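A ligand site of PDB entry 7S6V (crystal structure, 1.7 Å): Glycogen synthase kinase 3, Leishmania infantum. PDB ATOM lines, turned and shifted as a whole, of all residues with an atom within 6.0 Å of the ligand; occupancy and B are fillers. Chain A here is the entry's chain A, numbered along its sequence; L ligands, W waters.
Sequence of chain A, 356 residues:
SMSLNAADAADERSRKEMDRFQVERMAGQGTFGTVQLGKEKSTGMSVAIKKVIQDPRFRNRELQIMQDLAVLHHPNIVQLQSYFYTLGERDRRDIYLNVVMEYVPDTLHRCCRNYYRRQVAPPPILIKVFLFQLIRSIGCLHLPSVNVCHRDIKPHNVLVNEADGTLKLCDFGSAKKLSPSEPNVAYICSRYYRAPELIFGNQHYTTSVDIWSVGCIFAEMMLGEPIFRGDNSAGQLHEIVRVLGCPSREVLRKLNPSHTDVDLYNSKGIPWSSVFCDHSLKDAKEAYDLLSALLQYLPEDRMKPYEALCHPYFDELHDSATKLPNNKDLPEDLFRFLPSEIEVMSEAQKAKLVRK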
ATOM      1  N   ALA A  27      -5.654 -29.336 -24.210  1.00  0.00           N
ATOM      2  CA  ALA A  27      -4.685 -29.678 -25.255  1.00  0.00           C
ATOM      3  C   ALA A  27      -3.588 -30.539 -24.636  1.00  0.00           C
ATOM      4  O   ALA A  27      -3.209 -31.545 -25.204  1.00  0.00           O
ATOM      5  CB  ALA A  27      -4.082 -28.414 -25.867  1.00  0.00           C
ATOM      6  N   GLY A  28      -3.044 -30.101 -23.510  1.00  0.00           N
ATOM      7  CA  GLY A  28      -2.033 -30.877 -22.830  1.00  0.00           C
ATOM      8  C   GLY A  28      -1.848 -30.418 -21.402  1.00  0.00           C
ATOM      9  O   GLY A  28      -2.243 -29.324 -21.056  1.00  0.00           O
ATOM     10  N   GLN A  29      -1.210 -31.250 -20.591  1.00  0.00           N
ATOM     11  CA  GLN A  29      -0.956 -30.899 -19.211  1.00  0.00           C
ATOM     12  C   GLN A  29       0.314 -31.562 -18.726  1.00  0.00           C
ATOM     13  O   GLN A  29       0.774 -32.527 -19.343  1.00  0.00           O
ATOM     14  CB  GLN A  29      -2.144 -31.193 -18.291  1.00  0.00           C
ATOM     15  CG  GLN A  29      -2.710 -32.596 -18.356  1.00  0.00           C
ATOM     16  CD  GLN A  29      -4.039 -32.705 -17.638  1.00  0.00           C
ATOM     17  OE1 GLN A  29      -4.250 -32.079 -16.598  1.00  0.00           O
ATOM     18  NE2 GLN A  29      -4.951 -33.512 -18.184  1.00  0.00           N
ATOM     19  N   PHE A  32       4.491 -28.016 -16.153  1.00  0.00           N
ATOM     20  CA  PHE A  32       4.294 -26.562 -16.490  1.00  0.00           C
ATOM     21  C   PHE A  32       2.932 -26.005 -16.173  1.00  0.00           C
ATOM     22  O   PHE A  32       2.767 -24.820 -16.057  1.00  0.00           O
ATOM     23  CB  PHE A  32       4.478 -26.371 -18.014  1.00  0.00           C
ATOM     24  CG  PHE A  32       3.581 -27.242 -18.883  1.00  0.00           C
ATOM     25  CD1 PHE A  32       2.292 -26.838 -19.221  1.00  0.00           C
ATOM     26  CD2 PHE A  32       4.045 -28.442 -19.399  1.00  0.00           C
ATOM     27  CE1 PHE A  32       1.493 -27.633 -20.020  1.00  0.00           C
ATOM     28  CE2 PHE A  32       3.239 -29.230 -20.197  1.00  0.00           C
ATOM     29  CZ  PHE A  32       1.963 -28.819 -20.507  1.00  0.00           C
ATOM     30  N   THR A  34      -1.224 -26.373 -17.422  1.00  0.00           N
ATOM     31  CA  THR A  34      -2.139 -26.910 -18.357  1.00  0.00           C
ATOM     32  C   THR A  34      -2.320 -25.978 -19.513  1.00  0.00           C
ATOM     33  O   THR A  34      -2.140 -24.822 -19.336  1.00  0.00           O
ATOM     34  CB  THR A  34      -3.547 -27.156 -17.734  1.00  0.00           C
ATOM     35  OG1 THR A  34      -4.155 -25.898 -17.409  1.00  0.00           O
ATOM     36  CG2 THR A  34      -3.449 -27.969 -16.465  1.00  0.00           C
ATOM     37  N   VAL A  35      -2.600 -26.519 -20.693  1.00  0.00           N
ATOM     38  CA  VAL A  35      -2.874 -25.707 -21.847  1.00  0.00           C
ATOM     39  C   VAL A  35      -4.207 -26.158 -22.404  1.00  0.00           C
ATOM     40  O   VAL A  35      -4.344 -27.316 -22.736  1.00  0.00           O
ATOM     41  CB  VAL A  35      -1.796 -25.820 -22.949  1.00  0.00           C
ATOM     42  CG1 VAL A  35      -2.250 -25.102 -24.215  1.00  0.00           C
ATOM     43  CG2 VAL A  35      -0.477 -25.226 -22.470  1.00  0.00           C
ATOM     44  N   ALA A  48      -4.488 -20.732 -27.210  1.00  0.00           N
ATOM     45  CA  ALA A  48      -3.972 -21.667 -26.237  1.00  0.00           C
ATOM     46  C   ALA A  48      -4.045 -20.889 -24.911  1.00  0.00           C
ATOM     47  O   ALA A  48      -3.473 -19.819 -24.827  1.00  0.00           O
ATOM     48  CB  ALA A  48      -2.544 -22.028 -26.559  1.00  0.00           C
ATOM     49  N   LYS A  50      -2.961 -20.976 -21.191  1.00  0.00           N
ATOM     50  CA  LYS A  50      -2.015 -21.710 -20.371  1.00  0.00           C
ATOM     51  C   LYS A  50      -2.084 -21.297 -18.924  1.00  0.00           C
ATOM     52  O   LYS A  50      -1.803 -20.164 -18.637  1.00  0.00           O
ATOM     53  CB  LYS A  50      -0.585 -21.480 -20.846  1.00  0.00           C
ATOM     54  CG  LYS A  50       0.469 -22.242 -20.042  1.00  0.00           C
ATOM     55  CD  LYS A  50       1.864 -21.824 -20.456  1.00  0.00           C
ATOM     56  CE  LYS A  50       2.927 -22.585 -19.675  1.00  0.00           C
ATOM     57  NZ  LYS A  50       4.286 -22.023 -19.925  1.00  0.00           N
ATOM     58  N   GLU A  62       7.634 -15.132 -17.552  1.00  0.00           N
ATOM     59  CA  GLU A  62       6.736 -15.424 -18.655  1.00  0.00           C
ATOM     60  C   GLU A  62       5.924 -14.242 -19.114  1.00  0.00           C
ATOM     61  O   GLU A  62       5.908 -13.908 -20.302  1.00  0.00           O
ATOM     62  CB  GLU A  62       5.787 -16.544 -18.196  1.00  0.00           C
ATOM     63  CG  GLU A  62       4.536 -16.787 -19.018  1.00  0.00           C
ATOM     64  CD  GLU A  62       4.867 -17.434 -20.324  1.00  0.00           C
ATOM     65  OE1 GLU A  62       5.520 -16.752 -21.114  1.00  0.00           O
ATOM     66  OE2 GLU A  62       4.493 -18.609 -20.558  1.00  0.00           O
ATOM     67  N   VAL A  78       5.210 -16.895 -30.418  1.00  0.00           N
ATOM     68  CA  VAL A  78       3.819 -16.768 -29.982  1.00  0.00           C
ATOM     69  C   VAL A  78       3.486 -15.316 -29.578  1.00  0.00           C
ATOM     70  O   VAL A  78       4.343 -14.626 -29.050  1.00  0.00           O
ATOM     71  CB  VAL A  78       3.447 -17.750 -28.838  1.00  0.00           C
ATOM     72  CG1 VAL A  78       3.434 -19.194 -29.344  1.00  0.00           C
ATOM     73  CG2 VAL A  78       4.329 -17.589 -27.598  1.00  0.00           C
ATOM     74  N   VAL A  99      -1.873 -17.151 -19.266  1.00  0.00           N
ATOM     75  CA  VAL A  99      -1.519 -16.395 -20.489  1.00  0.00           C
ATOM     76  C   VAL A  99      -2.236 -17.007 -21.688  1.00  0.00           C
ATOM     77  O   VAL A  99      -2.322 -18.264 -21.837  1.00  0.00           O
ATOM     78  CB  VAL A  99       0.006 -16.263 -20.720  1.00  0.00           C
ATOM     79  CG1 VAL A  99       0.650 -15.355 -19.677  1.00  0.00           C
ATOM     80  CG2 VAL A  99       0.695 -17.565 -20.715  1.00  0.00           C
ATOM     81  N   MET A 101      -2.475 -17.089 -25.919  1.00  0.00           N
ATOM     82  CA  MET A 101      -1.740 -16.804 -27.152  1.00  0.00           C
ATOM     83  C   MET A 101      -2.443 -17.558 -28.272  1.00  0.00           C
ATOM     84  O   MET A 101      -3.360 -18.296 -28.025  1.00  0.00           O
ATOM     85  CB  MET A 101      -0.258 -17.177 -27.035  1.00  0.00           C
ATOM     86  CG  MET A 101       0.061 -18.629 -26.767  1.00  0.00           C
ATOM     87  SD  MET A 101       1.542 -18.701 -25.744  1.00  0.00           S
ATOM     88  CE  MET A 101       0.826 -18.567 -24.123  1.00  0.00           C
ATOM     89  N   GLU A 102      -2.009 -17.349 -29.506  1.00  0.00           N
ATOM     90  CA  GLU A 102      -2.590 -18.110 -30.604  1.00  0.00           C
ATOM     91  C   GLU A 102      -2.220 -19.577 -30.462  1.00  0.00           C
ATOM     92  O   GLU A 102      -1.153 -19.907 -29.968  1.00  0.00           O
ATOM     93  CB  GLU A 102      -2.222 -17.598 -31.996  1.00  0.00           C
ATOM     94  CG  GLU A 102      -0.801 -17.786 -32.480  1.00  0.00           C
ATOM     95  CD  GLU A 102       0.139 -16.751 -31.930  1.00  0.00           C
ATOM     96  OE1 GLU A 102      -0.267 -16.023 -31.007  1.00  0.00           O
ATOM     97  OE2 GLU A 102       1.267 -16.647 -32.394  1.00  0.00           O
ATOM     98  N   TYR A 103      -3.127 -20.443 -30.886  1.00  0.00           N
ATOM     99  CA  TYR A 103      -2.925 -21.878 -30.765  1.00  0.00           C
ATOM    100  C   TYR A 103      -2.070 -22.453 -31.867  1.00  0.00           C
ATOM    101  O   TYR A 103      -2.246 -22.080 -33.016  1.00  0.00           O
ATOM    102  CB  TYR A 103      -4.282 -22.548 -30.783  1.00  0.00           C
ATOM    103  CG  TYR A 103      -4.301 -24.041 -30.568  1.00  0.00           C
ATOM    104  CD1 TYR A 103      -4.150 -24.581 -29.301  1.00  0.00           C
ATOM    105  CD2 TYR A 103      -4.543 -24.908 -31.624  1.00  0.00           C
ATOM    106  CE1 TYR A 103      -4.203 -25.942 -29.098  1.00  0.00           C
ATOM    107  CE2 TYR A 103      -4.606 -26.263 -31.430  1.00  0.00           C
ATOM    108  CZ  TYR A 103      -4.442 -26.787 -30.165  1.00  0.00           C
ATOM    109  OH  TYR A 103      -4.502 -28.142 -29.961  1.00  0.00           O
ATOM    110  N   VAL A 104      -1.163 -23.364 -31.511  1.00  0.00           N
ATOM    111  CA  VAL A 104      -0.354 -24.065 -32.509  1.00  0.00           C
ATOM    112  C   VAL A 104      -0.686 -25.516 -32.220  1.00  0.00           C
ATOM    113  O   VAL A 104      -0.627 -25.925 -31.084  1.00  0.00           O
ATOM    114  CB  VAL A 104       1.154 -23.777 -32.365  1.00  0.00           C
ATOM    115  CG1 VAL A 104       1.935 -24.405 -33.520  1.00  0.00           C
ATOM    116  CG2 VAL A 104       1.414 -22.273 -32.298  1.00  0.00           C
ATOM    117  N   PRO A 105      -1.030 -26.305 -33.251  1.00  0.00           N
ATOM    118  CA  PRO A 105      -1.515 -27.675 -32.997  1.00  0.00           C
ATOM    119  C   PRO A 105      -0.599 -28.677 -32.325  1.00  0.00           C
ATOM    120  O   PRO A 105      -1.123 -29.540 -31.627  1.00  0.00           O
ATOM    121  CB  PRO A 105      -1.920 -28.177 -34.382  1.00  0.00           C
ATOM    122  CG  PRO A 105      -1.121 -27.384 -35.321  1.00  0.00           C
ATOM    123  CD  PRO A 105      -1.008 -26.028 -34.695  1.00  0.00           C
ATOM    124  N   ASP A 106       0.696 -28.630 -32.562  1.00  0.00           N
ATOM    125  CA  ASP A 106       1.590 -29.659 -32.050  1.00  0.00           C
ATOM    126  C   ASP A 106       2.936 -29.162 -31.609  1.00  0.00           C
ATOM    127  O   ASP A 106       3.296 -28.041 -31.907  1.00  0.00           O
ATOM    128  CB  ASP A 106       1.809 -30.693 -33.176  1.00  0.00           C
ATOM    129  CG  ASP A 106       2.159 -32.083 -32.669  1.00  0.00           C
ATOM    130  OD1 ASP A 106       1.970 -32.388 -31.473  1.00  0.00           O
ATOM    131  OD2 ASP A 106       2.615 -32.902 -33.501  1.00  0.00           O
ATOM    132  N   THR A 107       3.642 -29.981 -30.845  1.00  0.00           N
ATOM    133  CA  THR A 107       5.007 -29.650 -30.492  1.00  0.00           C
ATOM    134  C   THR A 107       5.922 -30.286 -31.515  1.00  0.00           C
ATOM    135  O   THR A 107       5.548 -31.262 -32.149  1.00  0.00           O
ATOM    136  CB  THR A 107       5.418 -30.217 -29.122  1.00  0.00           C
ATOM    137  OG1 THR A 107       5.246 -31.639 -29.128  1.00  0.00           O
ATOM    138  CG2 THR A 107       4.594 -29.599 -27.997  1.00  0.00           C
ATOM    139  N   HIS A 156       9.896 -29.638 -26.766  1.00  0.00           N
ATOM    140  CA  HIS A 156       8.574 -29.431 -26.172  1.00  0.00           C
ATOM    141  C   HIS A 156       8.049 -27.983 -26.205  1.00  0.00           C
ATOM    142  O   HIS A 156       6.844 -27.794 -26.132  1.00  0.00           O
ATOM    143  CB  HIS A 156       8.487 -30.017 -24.755  1.00  0.00           C
ATOM    144  CG  HIS A 156       8.149 -31.464 -24.731  1.00  0.00           C
ATOM    145  ND1 HIS A 156       9.107 -32.465 -24.738  1.00  0.00           N
ATOM    146  CD2 HIS A 156       6.952 -32.109 -24.746  1.00  0.00           C
ATOM    147  CE1 HIS A 156       8.521 -33.637 -24.726  1.00  0.00           C
ATOM    148  NE2 HIS A 156       7.210 -33.454 -24.731  1.00  0.00           N
ATOM    149  N   ASN A 157       8.908 -26.954 -26.304  1.00  0.00           N
ATOM    150  CA  ASN A 157       8.441 -25.516 -26.402  1.00  0.00           C
ATOM    151  C   ASN A 157       8.688 -24.947 -27.827  1.00  0.00           C
ATOM    152  O   ASN A 157       8.658 -23.762 -28.000  1.00  0.00           O
ATOM    153  CB  ASN A 157       8.918 -24.671 -25.258  1.00  0.00           C
ATOM    154  CG  ASN A 157      10.408 -24.611 -25.131  1.00  0.00           C
ATOM    155  OD1 ASN A 157      11.118 -24.666 -26.113  1.00  0.00           O
ATOM    156  ND2 ASN A 157      10.887 -24.469 -23.909  1.00  0.00           N
ATOM    157  N   LEU A 159       6.823 -25.130 -31.237  1.00  0.00           N
ATOM    158  CA  LEU A 159       5.515 -25.604 -31.666  1.00  0.00           C
ATOM    159  C   LEU A 159       5.441 -25.587 -33.160  1.00  0.00           C
ATOM    160  O   LEU A 159       6.074 -24.783 -33.751  1.00  0.00           O
ATOM    161  CB  LEU A 159       4.443 -24.700 -31.098  1.00  0.00           C
ATOM    162  CG  LEU A 159       4.524 -24.377 -29.595  1.00  0.00           C
ATOM    163  CD1 LEU A 159       3.438 -23.392 -29.218  1.00  0.00           C
ATOM    164  CD2 LEU A 159       4.468 -25.631 -28.733  1.00  0.00           C
ATOM    165  N   CYS A 170       7.811 -20.756 -27.981  1.00  0.00           N
ATOM    166  CA  CYS A 170       7.003 -20.335 -26.850  1.00  0.00           C
ATOM    167  C   CYS A 170       7.692 -20.677 -25.556  1.00  0.00           C
ATOM    168  O   CYS A 170       8.809 -21.156 -25.599  1.00  0.00           O
ATOM    169  CB  CYS A 170       5.651 -21.039 -26.890  1.00  0.00           C
ATOM    170  SG  CYS A 170       5.714 -22.755 -26.305  1.00  0.00           S
ATOM    171  N   ASP A 171       7.056 -20.401 -24.416  1.00  0.00           N
ATOM    172  CA  ASP A 171       7.582 -20.796 -23.094  1.00  0.00           C
ATOM    173  C   ASP A 171       8.729 -19.937 -22.614  1.00  0.00           C
ATOM    174  O   ASP A 171       9.842 -20.426 -22.522  1.00  0.00           O
ATOM    175  CB  ASP A 171       7.894 -22.294 -23.020  1.00  0.00           C
ATOM    176  CG  ASP A 171       8.114 -22.796 -21.604  1.00  0.00           C
ATOM    177  OD1 ASP A 171       7.787 -22.085 -20.629  1.00  0.00           O
ATOM    178  OD2 ASP A 171       8.627 -23.921 -21.464  1.00  0.00           O
ATOM    179  N   PHE A 172       8.445 -18.671 -22.335  1.00  0.00           N
ATOM    180  CA  PHE A 172       9.439 -17.751 -21.809  1.00  0.00           C
ATOM    181  C   PHE A 172       9.592 -17.566 -20.292  1.00  0.00           C
ATOM    182  O   PHE A 172      10.181 -16.586 -19.853  1.00  0.00           O
ATOM    183  CB  PHE A 172       9.195 -16.407 -22.496  1.00  0.00           C
ATOM    184  CG  PHE A 172       9.325 -16.469 -23.987  1.00  0.00           C
ATOM    185  CD1 PHE A 172      10.560 -16.298 -24.590  1.00  0.00           C
ATOM    186  CD2 PHE A 172       8.217 -16.710 -24.792  1.00  0.00           C
ATOM    187  CE1 PHE A 172      10.690 -16.362 -25.958  1.00  0.00           C
ATOM    188  CE2 PHE A 172       8.346 -16.774 -26.160  1.00  0.00           C
ATOM    189  CZ  PHE A 172       9.584 -16.603 -26.753  1.00  0.00           C
HETATM  190  C1  LIG L   1      -0.140 -29.579 -26.362  1.00  0.00           C
HETATM  191  C2  LIG L   1       2.722 -24.196 -24.578  1.00  0.00           C
HETATM  192  C3  LIG L   1      -0.472 -29.426 -27.680  1.00  0.00           C
HETATM  193  C4  LIG L   1      -0.535 -28.171 -28.246  1.00  0.00           C
HETATM  194  C5  LIG L   1       2.253 -23.066 -25.232  1.00  0.00           C
HETATM  195  C6  LIG L   1       0.109 -24.538 -27.779  1.00  0.00           C
HETATM  196  C7  LIG L   1       1.355 -23.186 -26.406  1.00  0.00           C
HETATM  197  C8  LIG L   1       0.227 -22.323 -28.282  1.00  0.00           C
HETATM  198  C9  LIG L   1       1.040 -22.093 -27.190  1.00  0.00           C
HETATM  199  C10 LIG L   1       3.514 -21.759 -23.688  1.00  0.00           C
HETATM  200  C11 LIG L   1       2.664 -21.836 -24.770  1.00  0.00           C
HETATM  201  N1  LIG L   1      -0.388 -25.776 -28.118  1.00  0.00           N
HETATM  202  N2  LIG L   1       0.904 -24.415 -26.704  1.00  0.00           N
HETATM  203  C12 LIG L   1       0.108 -28.457 -25.604  1.00  0.00           C
HETATM  204  N3  LIG L   1      -0.258 -23.525 -28.592  1.00  0.00           N
HETATM  205  C13 LIG L   1      -0.286 -27.036 -27.479  1.00  0.00           C
HETATM  206  C14 LIG L   1       0.047 -27.182 -26.130  1.00  0.00           C
HETATM  207 CL1  LIG L   1       0.528 -28.654 -23.937  1.00  0.00          CL
HETATM  208  N4  LIG L   1       3.971 -22.840 -23.040  1.00  0.00           N
HETATM  209  C15 LIG L   1       3.586 -24.048 -23.478  1.00  0.00           C
HETATM  210  N5  LIG L   1       4.069 -25.107 -22.806  1.00  0.00           N
HETATM  211  C16 LIG L   1       3.779 -26.487 -23.112  1.00  0.00           C
HETATM  212  C17 LIG L   1       4.300 -26.909 -24.472  1.00  0.00           C
HETATM  213  C18 LIG L   1       4.066 -28.364 -24.781  1.00  0.00           C
HETATM  214  O1  LIG L   1       4.866 -29.213 -23.968  1.00  0.00           O
HETATM  215  O   HOH W   1       4.836 -18.554 -23.683  1.00  0.00           O
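Water W1 bridges the backbone NH of Asp 171 (3.0 Å) and the side-chain carboxylate of Glu 62 (3.1 Å).
Residues that only touch the ligand: Glu 102 (3.3 Å), Ala 48 (3.3 Å), Leu 159 (3.4 Å), Met 101 (3.5 Å), Thr 107 (3.5 Å), Gly 28 (3.6 Å), Val 35 (3.6 Å), Pro 105 (3.7 Å), Phe 32 (3.7 Å), Tyr 103 (3.8 Å), Ala 27 (3.8 Å) and Asp 171 (3.9 Å). Of the 24 residues printed, 16 come within 4 Å of the ligand.
The backbone NH (N) of Val 104 is in hydrogen-bond range of a nitrogen (N3) of the ligand (3.1 Å). The backbone carbonyl oxygen of Val 104 lies within hydrogen-bond range of a nitrogen (N1) of the ligand. The backbone carbonyl oxygen of His 156 lies close to an oxygen (O1) of the ligand, at 3.3 Å. N4 of the ligand lies within hydrogen-bond range of NZ of Lys 50 (3.2 Å). A nitrogen (N4) of the ligand sits close to the side-chain sulfur (SG) of Cys 170.
The side-chain amino group of Lys 50 is in salt-bridge range of the side-chain carboxylate of Asp 171, 3.6 Å away. OE2 of Glu 62 is in salt-bridge range of NZ of Lys 50, at 3.5 Å. O of Val 99 is in hydrogen-bond range of N of Lys 50, at 2.9 Å. O of Met 101 lies within hydrogen-bond range of N of Ala 48. N of Cys 170 lies within hydrogen-bond range of O of Asn 157, 3.1 Å away. The backbone carbonyl oxygen (O) of Gly 28 is in hydrogen-bond range of the backbone NH (N) of Val 35, at 2.9 Å. The backbone NH (N) of Ala 27 sits at hydrogen-bond distance from the backbone carbonyl oxygen (O) of Val 35, 2.8 Å away. The side-chain carboxylate of Asp 171 is in hydrogen-bond range of the side-chain amide nitrogen of Asn 157 (3.4 Å).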
